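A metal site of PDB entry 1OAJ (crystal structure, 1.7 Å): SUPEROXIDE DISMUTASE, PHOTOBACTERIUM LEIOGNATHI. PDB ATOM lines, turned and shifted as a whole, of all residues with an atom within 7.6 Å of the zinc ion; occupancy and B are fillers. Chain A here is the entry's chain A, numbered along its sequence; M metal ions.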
ATOM      1  N   PHE A  44     -32.600  21.867  -3.913  1.00  0.00           N
ATOM      2  CA  PHE A  44     -32.733  22.094  -2.481  1.00  0.00           C
ATOM      3  C   PHE A  44     -31.556  22.932  -2.016  1.00  0.00           C
ATOM      4  O   PHE A  44     -30.450  22.425  -1.897  1.00  0.00           O
ATOM      5  CB  PHE A  44     -32.735  20.744  -1.790  1.00  0.00           C
ATOM      6  CG  PHE A  44     -33.161  20.709  -0.359  1.00  0.00           C
ATOM      7  CD1 PHE A  44     -34.161  21.520   0.112  1.00  0.00           C
ATOM      8  CD2 PHE A  44     -32.513  19.858   0.528  1.00  0.00           C
ATOM      9  CE1 PHE A  44     -34.515  21.467   1.445  1.00  0.00           C
ATOM     10  CE2 PHE A  44     -32.878  19.801   1.842  1.00  0.00           C
ATOM     11  CZ  PHE A  44     -33.883  20.600   2.308  1.00  0.00           C
ATOM     12  N   HIS A  45     -31.755  24.223  -1.742  1.00  0.00           N
ATOM     13  CA  HIS A  45     -30.616  25.050  -1.290  1.00  0.00           C
ATOM     14  C   HIS A  45     -30.961  26.086  -0.251  1.00  0.00           C
ATOM     15  O   HIS A  45     -32.107  26.459  -0.049  1.00  0.00           O
ATOM     16  CB  HIS A  45     -30.016  25.808  -2.453  1.00  0.00           C
ATOM     17  CG  HIS A  45     -30.335  25.241  -3.841  1.00  0.00           C
ATOM     18  ND1 HIS A  45     -31.265  25.785  -4.692  1.00  0.00           N
ATOM     19  CD2 HIS A  45     -29.815  24.173  -4.483  1.00  0.00           C
ATOM     20  CE1 HIS A  45     -31.306  25.069  -5.818  1.00  0.00           C
ATOM     21  NE2 HIS A  45     -30.435  24.078  -5.709  1.00  0.00           N
ATOM     22  N   ILE A  46     -29.931  26.540   0.452  1.00  0.00           N
ATOM     23  CA  ILE A  46     -30.100  27.645   1.385  1.00  0.00           C
ATOM     24  C   ILE A  46     -29.976  28.882   0.547  1.00  0.00           C
ATOM     25  O   ILE A  46     -29.082  28.993  -0.285  1.00  0.00           O
ATOM     26  CB  ILE A  46     -28.990  27.699   2.460  1.00  0.00           C
ATOM     27  CG1 ILE A  46     -28.872  26.351   3.193  1.00  0.00           C
ATOM     28  CG2 ILE A  46     -29.244  28.818   3.458  1.00  0.00           C
ATOM     29  CD1 ILE A  46     -30.183  25.590   3.294  1.00  0.00           C
ATOM     30  N   HIS A  47     -30.904  29.827   0.744  1.00  0.00           N
ATOM     31  CA  HIS A  47     -30.837  31.077   0.002  1.00  0.00           C
ATOM     32  C   HIS A  47     -30.404  32.192   0.944  1.00  0.00           C
ATOM     33  O   HIS A  47     -30.529  32.064   2.155  1.00  0.00           O
ATOM     34  CB  HIS A  47     -32.162  31.366  -0.687  1.00  0.00           C
ATOM     35  CG  HIS A  47     -32.297  30.621  -2.046  1.00  0.00           C
ATOM     36  ND1 HIS A  47     -32.404  31.300  -3.234  1.00  0.00           N
ATOM     37  CD2 HIS A  47     -32.352  29.284  -2.347  1.00  0.00           C
ATOM     38  CE1 HIS A  47     -32.516  30.420  -4.220  1.00  0.00           C
ATOM     39  NE2 HIS A  47     -32.490  29.200  -3.701  1.00  0.00           N
ATOM     40  N   GLY A  69     -30.444  35.047  -3.849  1.00  0.00           N
ATOM     41  CA  GLY A  69     -29.832  33.955  -4.578  1.00  0.00           C
ATOM     42  C   GLY A  69     -29.295  32.948  -3.586  1.00  0.00           C
ATOM     43  O   GLY A  69     -29.616  33.039  -2.385  1.00  0.00           O
ATOM     44  N   HIS A  70     -28.490  32.006  -4.042  1.00  0.00           N
ATOM     45  CA  HIS A  70     -27.955  31.004  -3.123  1.00  0.00           C
ATOM     46  C   HIS A  70     -27.005  31.583  -2.101  1.00  0.00           C
ATOM     47  O   HIS A  70     -26.247  32.521  -2.401  1.00  0.00           O
ATOM     48  CB  HIS A  70     -27.248  29.893  -3.874  1.00  0.00           C
ATOM     49  CG  HIS A  70     -28.194  29.036  -4.742  1.00  0.00           C
ATOM     50  ND1 HIS A  70     -27.788  27.905  -5.428  1.00  0.00           N
ATOM     51  CD2 HIS A  70     -29.515  29.168  -5.002  1.00  0.00           C
ATOM     52  CE1 HIS A  70     -28.803  27.395  -6.091  1.00  0.00           C
ATOM     53  NE2 HIS A  70     -29.867  28.143  -5.847  1.00  0.00           N
ATOM     54  N   TYR A  71     -27.040  31.024  -0.886  1.00  0.00           N
ATOM     55  CA  TYR A  71     -26.143  31.387   0.200  1.00  0.00           C
ATOM     56  C   TYR A  71     -24.750  31.168  -0.341  1.00  0.00           C
ATOM     57  O   TYR A  71     -24.455  30.100  -0.889  1.00  0.00           O
ATOM     58  CB  TYR A  71     -26.485  30.586   1.442  1.00  0.00           C
ATOM     59  CG  TYR A  71     -25.576  30.815   2.642  1.00  0.00           C
ATOM     60  CD1 TYR A  71     -25.312  32.093   3.120  1.00  0.00           C
ATOM     61  CD2 TYR A  71     -25.013  29.718   3.270  1.00  0.00           C
ATOM     62  CE1 TYR A  71     -24.466  32.237   4.211  1.00  0.00           C
ATOM     63  CE2 TYR A  71     -24.201  29.864   4.375  1.00  0.00           C
ATOM     64  CZ  TYR A  71     -23.940  31.129   4.826  1.00  0.00           C
ATOM     65  OH  TYR A  71     -23.141  31.292   5.924  1.00  0.00           O
ATOM     66  N   ASP A  72     -23.891  32.161  -0.210  1.00  0.00           N
ATOM     67  CA  ASP A  72     -22.574  32.091  -0.869  1.00  0.00           C
ATOM     68  C   ASP A  72     -21.578  32.962  -0.135  1.00  0.00           C
ATOM     69  O   ASP A  72     -21.053  33.950  -0.665  1.00  0.00           O
ATOM     70  CB  ASP A  72     -22.784  32.500  -2.318  1.00  0.00           C
ATOM     71  CG  ASP A  72     -21.568  32.410  -3.187  1.00  0.00           C
ATOM     72  OD1 ASP A  72     -20.700  31.554  -2.912  1.00  0.00           O
ATOM     73  OD2 ASP A  72     -21.452  33.192  -4.160  1.00  0.00           O
ATOM     74  N   THR A  76     -18.294  32.833  -4.249  1.00  0.00           N
ATOM     75  CA  THR A  76     -17.854  31.981  -5.363  1.00  0.00           C
ATOM     76  C   THR A  76     -18.561  32.295  -6.642  1.00  0.00           C
ATOM     77  O   THR A  76     -17.968  32.261  -7.720  1.00  0.00           O
ATOM     78  CB  THR A  76     -18.072  30.520  -5.039  1.00  0.00           C
ATOM     79  OG1 THR A  76     -19.492  30.270  -4.911  1.00  0.00           O
ATOM     80  CG2 THR A  76     -17.363  30.145  -3.754  1.00  0.00           C
ATOM     81  N   LYS A  78     -20.791  30.565  -8.096  1.00  0.00           N
ATOM     82  CA  LYS A  78     -20.896  29.349  -8.871  1.00  0.00           C
ATOM     83  C   LYS A  78     -21.768  28.337  -8.150  1.00  0.00           C
ATOM     84  O   LYS A  78     -21.790  28.301  -6.911  1.00  0.00           O
ATOM     85  CB  LYS A  78     -19.506  28.725  -9.119  1.00  0.00           C
ATOM     86  CG  LYS A  78     -18.466  29.691  -9.627  1.00  0.00           C
ATOM     87  CD  LYS A  78     -17.051  29.155  -9.419  1.00  0.00           C
ATOM     88  CE  LYS A  78     -16.164  29.468 -10.606  1.00  0.00           C
ATOM     89  NZ  LYS A  78     -16.243  30.901 -10.994  1.00  0.00           N
ATOM     90  N   HIS A  79     -22.479  27.527  -8.908  1.00  0.00           N
ATOM     91  CA  HIS A  79     -23.363  26.522  -8.338  1.00  0.00           C
ATOM     92  C   HIS A  79     -22.666  25.171  -8.473  1.00  0.00           C
ATOM     93  O   HIS A  79     -22.164  24.854  -9.567  1.00  0.00           O
ATOM     94  CB  HIS A  79     -24.736  26.571  -9.034  1.00  0.00           C
ATOM     95  CG  HIS A  79     -25.658  25.527  -8.445  1.00  0.00           C
ATOM     96  ND1 HIS A  79     -26.290  25.684  -7.236  1.00  0.00           N
ATOM     97  CD2 HIS A  79     -26.052  24.310  -8.905  1.00  0.00           C
ATOM     98  CE1 HIS A  79     -27.010  24.610  -6.949  1.00  0.00           C
ATOM     99  NE2 HIS A  79     -26.895  23.756  -7.952  1.00  0.00           N
ATOM    100  N   GLY A  80     -22.601  24.369  -7.409  1.00  0.00           N
ATOM    101  CA  GLY A  80     -21.926  23.098  -7.492  1.00  0.00           C
ATOM    102  C   GLY A  80     -22.517  22.069  -6.554  1.00  0.00           C
ATOM    103  O   GLY A  80     -23.720  22.071  -6.270  1.00  0.00           O
ATOM    104  N   PHE A  81     -21.649  21.205  -6.075  1.00  0.00           N
ATOM    105  CA  PHE A  81     -22.061  20.122  -5.229  1.00  0.00           C
ATOM    106  C   PHE A  81     -21.941  20.447  -3.754  1.00  0.00           C
ATOM    107  O   PHE A  81     -21.329  21.465  -3.399  1.00  0.00           O
ATOM    108  CB  PHE A  81     -21.160  18.911  -5.434  1.00  0.00           C
ATOM    109  CG  PHE A  81     -21.164  18.334  -6.786  1.00  0.00           C
ATOM    110  CD1 PHE A  81     -22.065  17.318  -7.101  1.00  0.00           C
ATOM    111  CD2 PHE A  81     -20.259  18.791  -7.732  1.00  0.00           C
ATOM    112  CE1 PHE A  81     -22.084  16.795  -8.363  1.00  0.00           C
ATOM    113  CE2 PHE A  81     -20.276  18.258  -8.993  1.00  0.00           C
ATOM    114  CZ  PHE A  81     -21.206  17.246  -9.303  1.00  0.00           C
ATOM    115  N   ASN A  87     -18.029  26.807  -4.746  1.00  0.00           N
ATOM    116  CA  ASN A  87     -19.403  27.061  -5.147  1.00  0.00           C
ATOM    117  C   ASN A  87     -20.213  27.403  -3.904  1.00  0.00           C
ATOM    118  O   ASN A  87     -19.720  27.272  -2.794  1.00  0.00           O
ATOM    119  CB  ASN A  87     -19.985  25.899  -5.940  1.00  0.00           C
ATOM    120  CG  ASN A  87     -19.936  24.573  -5.225  1.00  0.00           C
ATOM    121  OD1 ASN A  87     -18.988  23.810  -5.403  1.00  0.00           O
ATOM    122  ND2 ASN A  87     -20.967  24.291  -4.427  1.00  0.00           N
ATOM    123  N   HIS A  88     -21.448  27.862  -4.087  1.00  0.00           N
ATOM    124  CA  HIS A  88     -22.299  28.246  -2.986  1.00  0.00           C
ATOM    125  C   HIS A  88     -22.350  27.254  -1.849  1.00  0.00           C
ATOM    126  O   HIS A  88     -22.688  26.088  -2.065  1.00  0.00           O
ATOM    127  CB  HIS A  88     -23.746  28.384  -3.447  1.00  0.00           C
ATOM    128  CG  HIS A  88     -23.955  29.099  -4.793  1.00  0.00           C
ATOM    129  ND1 HIS A  88     -24.815  28.639  -5.780  1.00  0.00           N
ATOM    130  CD2 HIS A  88     -23.441  30.266  -5.240  1.00  0.00           C
ATOM    131  CE1 HIS A  88     -24.795  29.477  -6.785  1.00  0.00           C
ATOM    132  NE2 HIS A  88     -23.974  30.482  -6.475  1.00  0.00           N
ATOM    133  N   LYS A  89     -22.027  27.715  -0.660  1.00  0.00           N
ATOM    134  CA  LYS A  89     -22.102  26.865   0.523  1.00  0.00           C
ATOM    135  C   LYS A  89     -23.538  26.431   0.756  1.00  0.00           C
ATOM    136  O   LYS A  89     -23.827  25.440   1.415  1.00  0.00           O
ATOM    137  CB  LYS A  89     -21.581  27.628   1.764  1.00  0.00           C
ATOM    138  CG  LYS A  89     -20.557  26.900   2.597  1.00  0.00           C
ATOM    139  CD  LYS A  89     -19.859  27.836   3.575  1.00  0.00           C
ATOM    140  CE  LYS A  89     -18.397  27.493   3.701  1.00  0.00           C
ATOM    141  NZ  LYS A  89     -17.961  27.388   5.123  1.00  0.00           N
ATOM    142  N   GLY A  90     -24.445  27.195   0.158  1.00  0.00           N
ATOM    143  CA  GLY A  90     -25.851  26.898   0.304  1.00  0.00           C
ATOM    144  C   GLY A  90     -26.285  25.651  -0.449  1.00  0.00           C
ATOM    145  O   GLY A  90     -27.360  25.117  -0.172  1.00  0.00           O
ATOM    146  N   ASP A  91     -25.467  25.145  -1.392  1.00  0.00           N
ATOM    147  CA  ASP A  91     -25.833  23.973  -2.225  1.00  0.00           C
ATOM    148  C   ASP A  91     -25.990  22.650  -1.465  1.00  0.00           C
ATOM    149  O   ASP A  91     -25.000  22.086  -0.985  1.00  0.00           O
ATOM    150  CB  ASP A  91     -24.811  23.817  -3.347  1.00  0.00           C
ATOM    151  CG  ASP A  91     -24.764  25.053  -4.236  1.00  0.00           C
ATOM    152  OD1 ASP A  91     -25.770  25.797  -4.277  1.00  0.00           O
ATOM    153  OD2 ASP A  91     -23.725  25.274  -4.891  1.00  0.00           O
ATOM    154  N   LEU A  92     -27.222  22.188  -1.354  1.00  0.00           N
ATOM    155  CA  LEU A  92     -27.511  20.953  -0.623  1.00  0.00           C
ATOM    156  C   LEU A  92     -27.750  19.754  -1.556  1.00  0.00           C
ATOM    157  O   LEU A  92     -27.966  19.951  -2.754  1.00  0.00           O
ATOM    158  CB  LEU A  92     -28.735  21.155   0.264  1.00  0.00           C
ATOM    159  CG  LEU A  92     -28.826  22.476   1.043  1.00  0.00           C
ATOM    160  CD1 LEU A  92     -30.277  22.771   1.397  1.00  0.00           C
ATOM    161  CD2 LEU A  92     -27.947  22.431   2.280  1.00  0.00           C
ATOM    162  N   ARG A 111     -20.519  20.935   4.495  1.00  0.00           N
ATOM    163  CA  ARG A 111     -19.824  22.221   4.536  1.00  0.00           C
ATOM    164  C   ARG A 111     -20.509  23.294   5.418  1.00  0.00           C
ATOM    165  O   ARG A 111     -19.915  24.323   5.703  1.00  0.00           O
ATOM    166  CB  ARG A 111     -19.687  22.762   3.124  1.00  0.00           C
ATOM    167  CG  ARG A 111     -18.731  21.985   2.244  1.00  0.00           C
ATOM    168  CD  ARG A 111     -18.383  22.767   1.003  1.00  0.00           C
ATOM    169  NE  ARG A 111     -19.521  22.851   0.092  1.00  0.00           N
ATOM    170  CZ  ARG A 111     -19.904  23.939  -0.576  1.00  0.00           C
ATOM    171  NH1 ARG A 111     -19.229  25.070  -0.455  1.00  0.00           N
ATOM    172  NH2 ARG A 111     -20.970  23.903  -1.392  1.00  0.00           N
ATOM    173  N   ASP A 129     -31.543  19.179  -9.668  1.00  0.00           N
ATOM    174  CA  ASP A 129     -30.274  19.859  -9.434  1.00  0.00           C
ATOM    175  C   ASP A 129     -29.093  19.010  -9.935  1.00  0.00           C
ATOM    176  O   ASP A 129     -28.686  18.053  -9.251  1.00  0.00           O
ATOM    177  CB  ASP A 129     -30.112  20.144  -7.948  1.00  0.00           C
ATOM    178  CG  ASP A 129     -28.963  21.097  -7.657  1.00  0.00           C
ATOM    179  OD1 ASP A 129     -28.115  21.296  -8.534  1.00  0.00           O
ATOM    180  OD2 ASP A 129     -28.915  21.649  -6.542  1.00  0.00           O
ATOM    181  N   HIS A 131     -26.195  19.987 -10.085  1.00  0.00           N
ATOM    182  CA  HIS A 131     -25.038  20.592  -9.452  1.00  0.00           C
ATOM    183  C   HIS A 131     -24.055  21.192 -10.429  1.00  0.00           C
ATOM    184  O   HIS A 131     -22.849  20.943 -10.388  1.00  0.00           O
ATOM    185  CB  HIS A 131     -24.323  19.573  -8.550  1.00  0.00           C
ATOM    186  CG  HIS A 131     -25.268  19.088  -7.405  1.00  0.00           C
ATOM    187  ND1 HIS A 131     -25.966  17.895  -7.427  1.00  0.00           N
ATOM    188  CD2 HIS A 131     -25.633  19.692  -6.254  1.00  0.00           C
ATOM    189  CE1 HIS A 131     -26.739  17.800  -6.358  1.00  0.00           C
ATOM    190  NE2 HIS A 131     -26.549  18.869  -5.626  1.00  0.00           N
ATOM    191  N   ASP A 133     -23.940  24.804 -13.456  1.00  0.00           N
ATOM    192  CA  ASP A 133     -24.642  25.920 -14.052  1.00  0.00           C
ATOM    193  C   ASP A 133     -24.877  25.586 -15.519  1.00  0.00           C
ATOM    194  O   ASP A 133     -25.318  26.457 -16.282  1.00  0.00           O
ATOM    195  CB  ASP A 133     -23.878  27.224 -13.845  1.00  0.00           C
ATOM    196  CG  ASP A 133     -24.094  27.789 -12.458  1.00  0.00           C
ATOM    197  OD1 ASP A 133     -25.269  27.991 -12.065  1.00  0.00           O
ATOM    198  OD2 ASP A 133     -23.086  28.050 -11.765  1.00  0.00           O
ATOM    199  N   LEU A 138     -28.040  27.430 -12.067  1.00  0.00           N
ATOM    200  CA  LEU A 138     -28.398  26.917 -10.782  1.00  0.00           C
ATOM    201  C   LEU A 138     -28.915  25.496 -10.733  1.00  0.00           C
ATOM    202  O   LEU A 138     -29.894  25.210 -10.045  1.00  0.00           O
ATOM    203  CB  LEU A 138     -29.366  27.902 -10.141  1.00  0.00           C
ATOM    204  CG  LEU A 138     -28.844  29.333 -10.222  1.00  0.00           C
ATOM    205  CD1 LEU A 138     -29.974  30.329 -10.044  1.00  0.00           C
ATOM    206  CD2 LEU A 138     -27.768  29.552  -9.189  1.00  0.00           C
ATOM    207  N   GLY A 139     -28.260  24.602 -11.448  1.00  0.00           N
ATOM    208  CA  GLY A 139     -28.605  23.179 -11.467  1.00  0.00           C
ATOM    209  C   GLY A 139     -29.938  22.845 -12.163  1.00  0.00           C
ATOM    210  O   GLY A 139     -30.342  21.678 -12.135  1.00  0.00           O
HETATM  211 ZN    ZN M   1     -26.039  27.071  -5.690  1.00  0.00          ZN
HETATM  212 CU    CU M   2     -32.347  27.520  -4.636  1.00  0.00          CU
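Four residues have an atom within 4 Å of the zinc ion: His 70, His 79, His 88 and Asp 91. Along chain A the residues within 4 Å of the zinc ion span positions 70 to 91. The nearest printed residue that does not touch the zinc ion is Lys 78 (4.6 Å).
OG1 of Thr 76 is in hydrogen-bond range of N of His 88, at 3.2 Å. A ring nitrogen (ND1) of His 45 sits close to a ring nitrogen (NE2) of His 70 (3.0 Å). O of His 88 lies within hydrogen-bond range of NH2 of Arg 111 (2.9 Å). N of Gly 80 sits at hydrogen-bond distance from OD2 of Asp 91, at 2.9 Å. The side-chain carboxylate (OD1) of Asp 129 lies within hydrogen-bond range of a ring nitrogen (NE2) of His 79. The side-chain amide nitrogen of Asn 87 lies within hydrogen-bond range of the side-chain carboxylate of Asp 91, 3.0 Å away. The backbone NH of His 79 sits at hydrogen-bond distance from the side-chain carboxylate of Asp 133, at 3.0 Å. The backbone NH (N) of His 88 lies within hydrogen-bond range of the backbone carbonyl oxygen (O) of Lys 78, at 2.9 Å.
OD1 of Asp 91 binds the zinc ion (1.9 Å). A ring nitrogen (ND1) of His 70 binds the zinc ion, 2.0 Å away. ND1 of His 88 binds the zinc ion (2.0 Å). ND1 of His 79 is bound to the zinc ion. The zinc ion has four donor atoms within binding distance.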
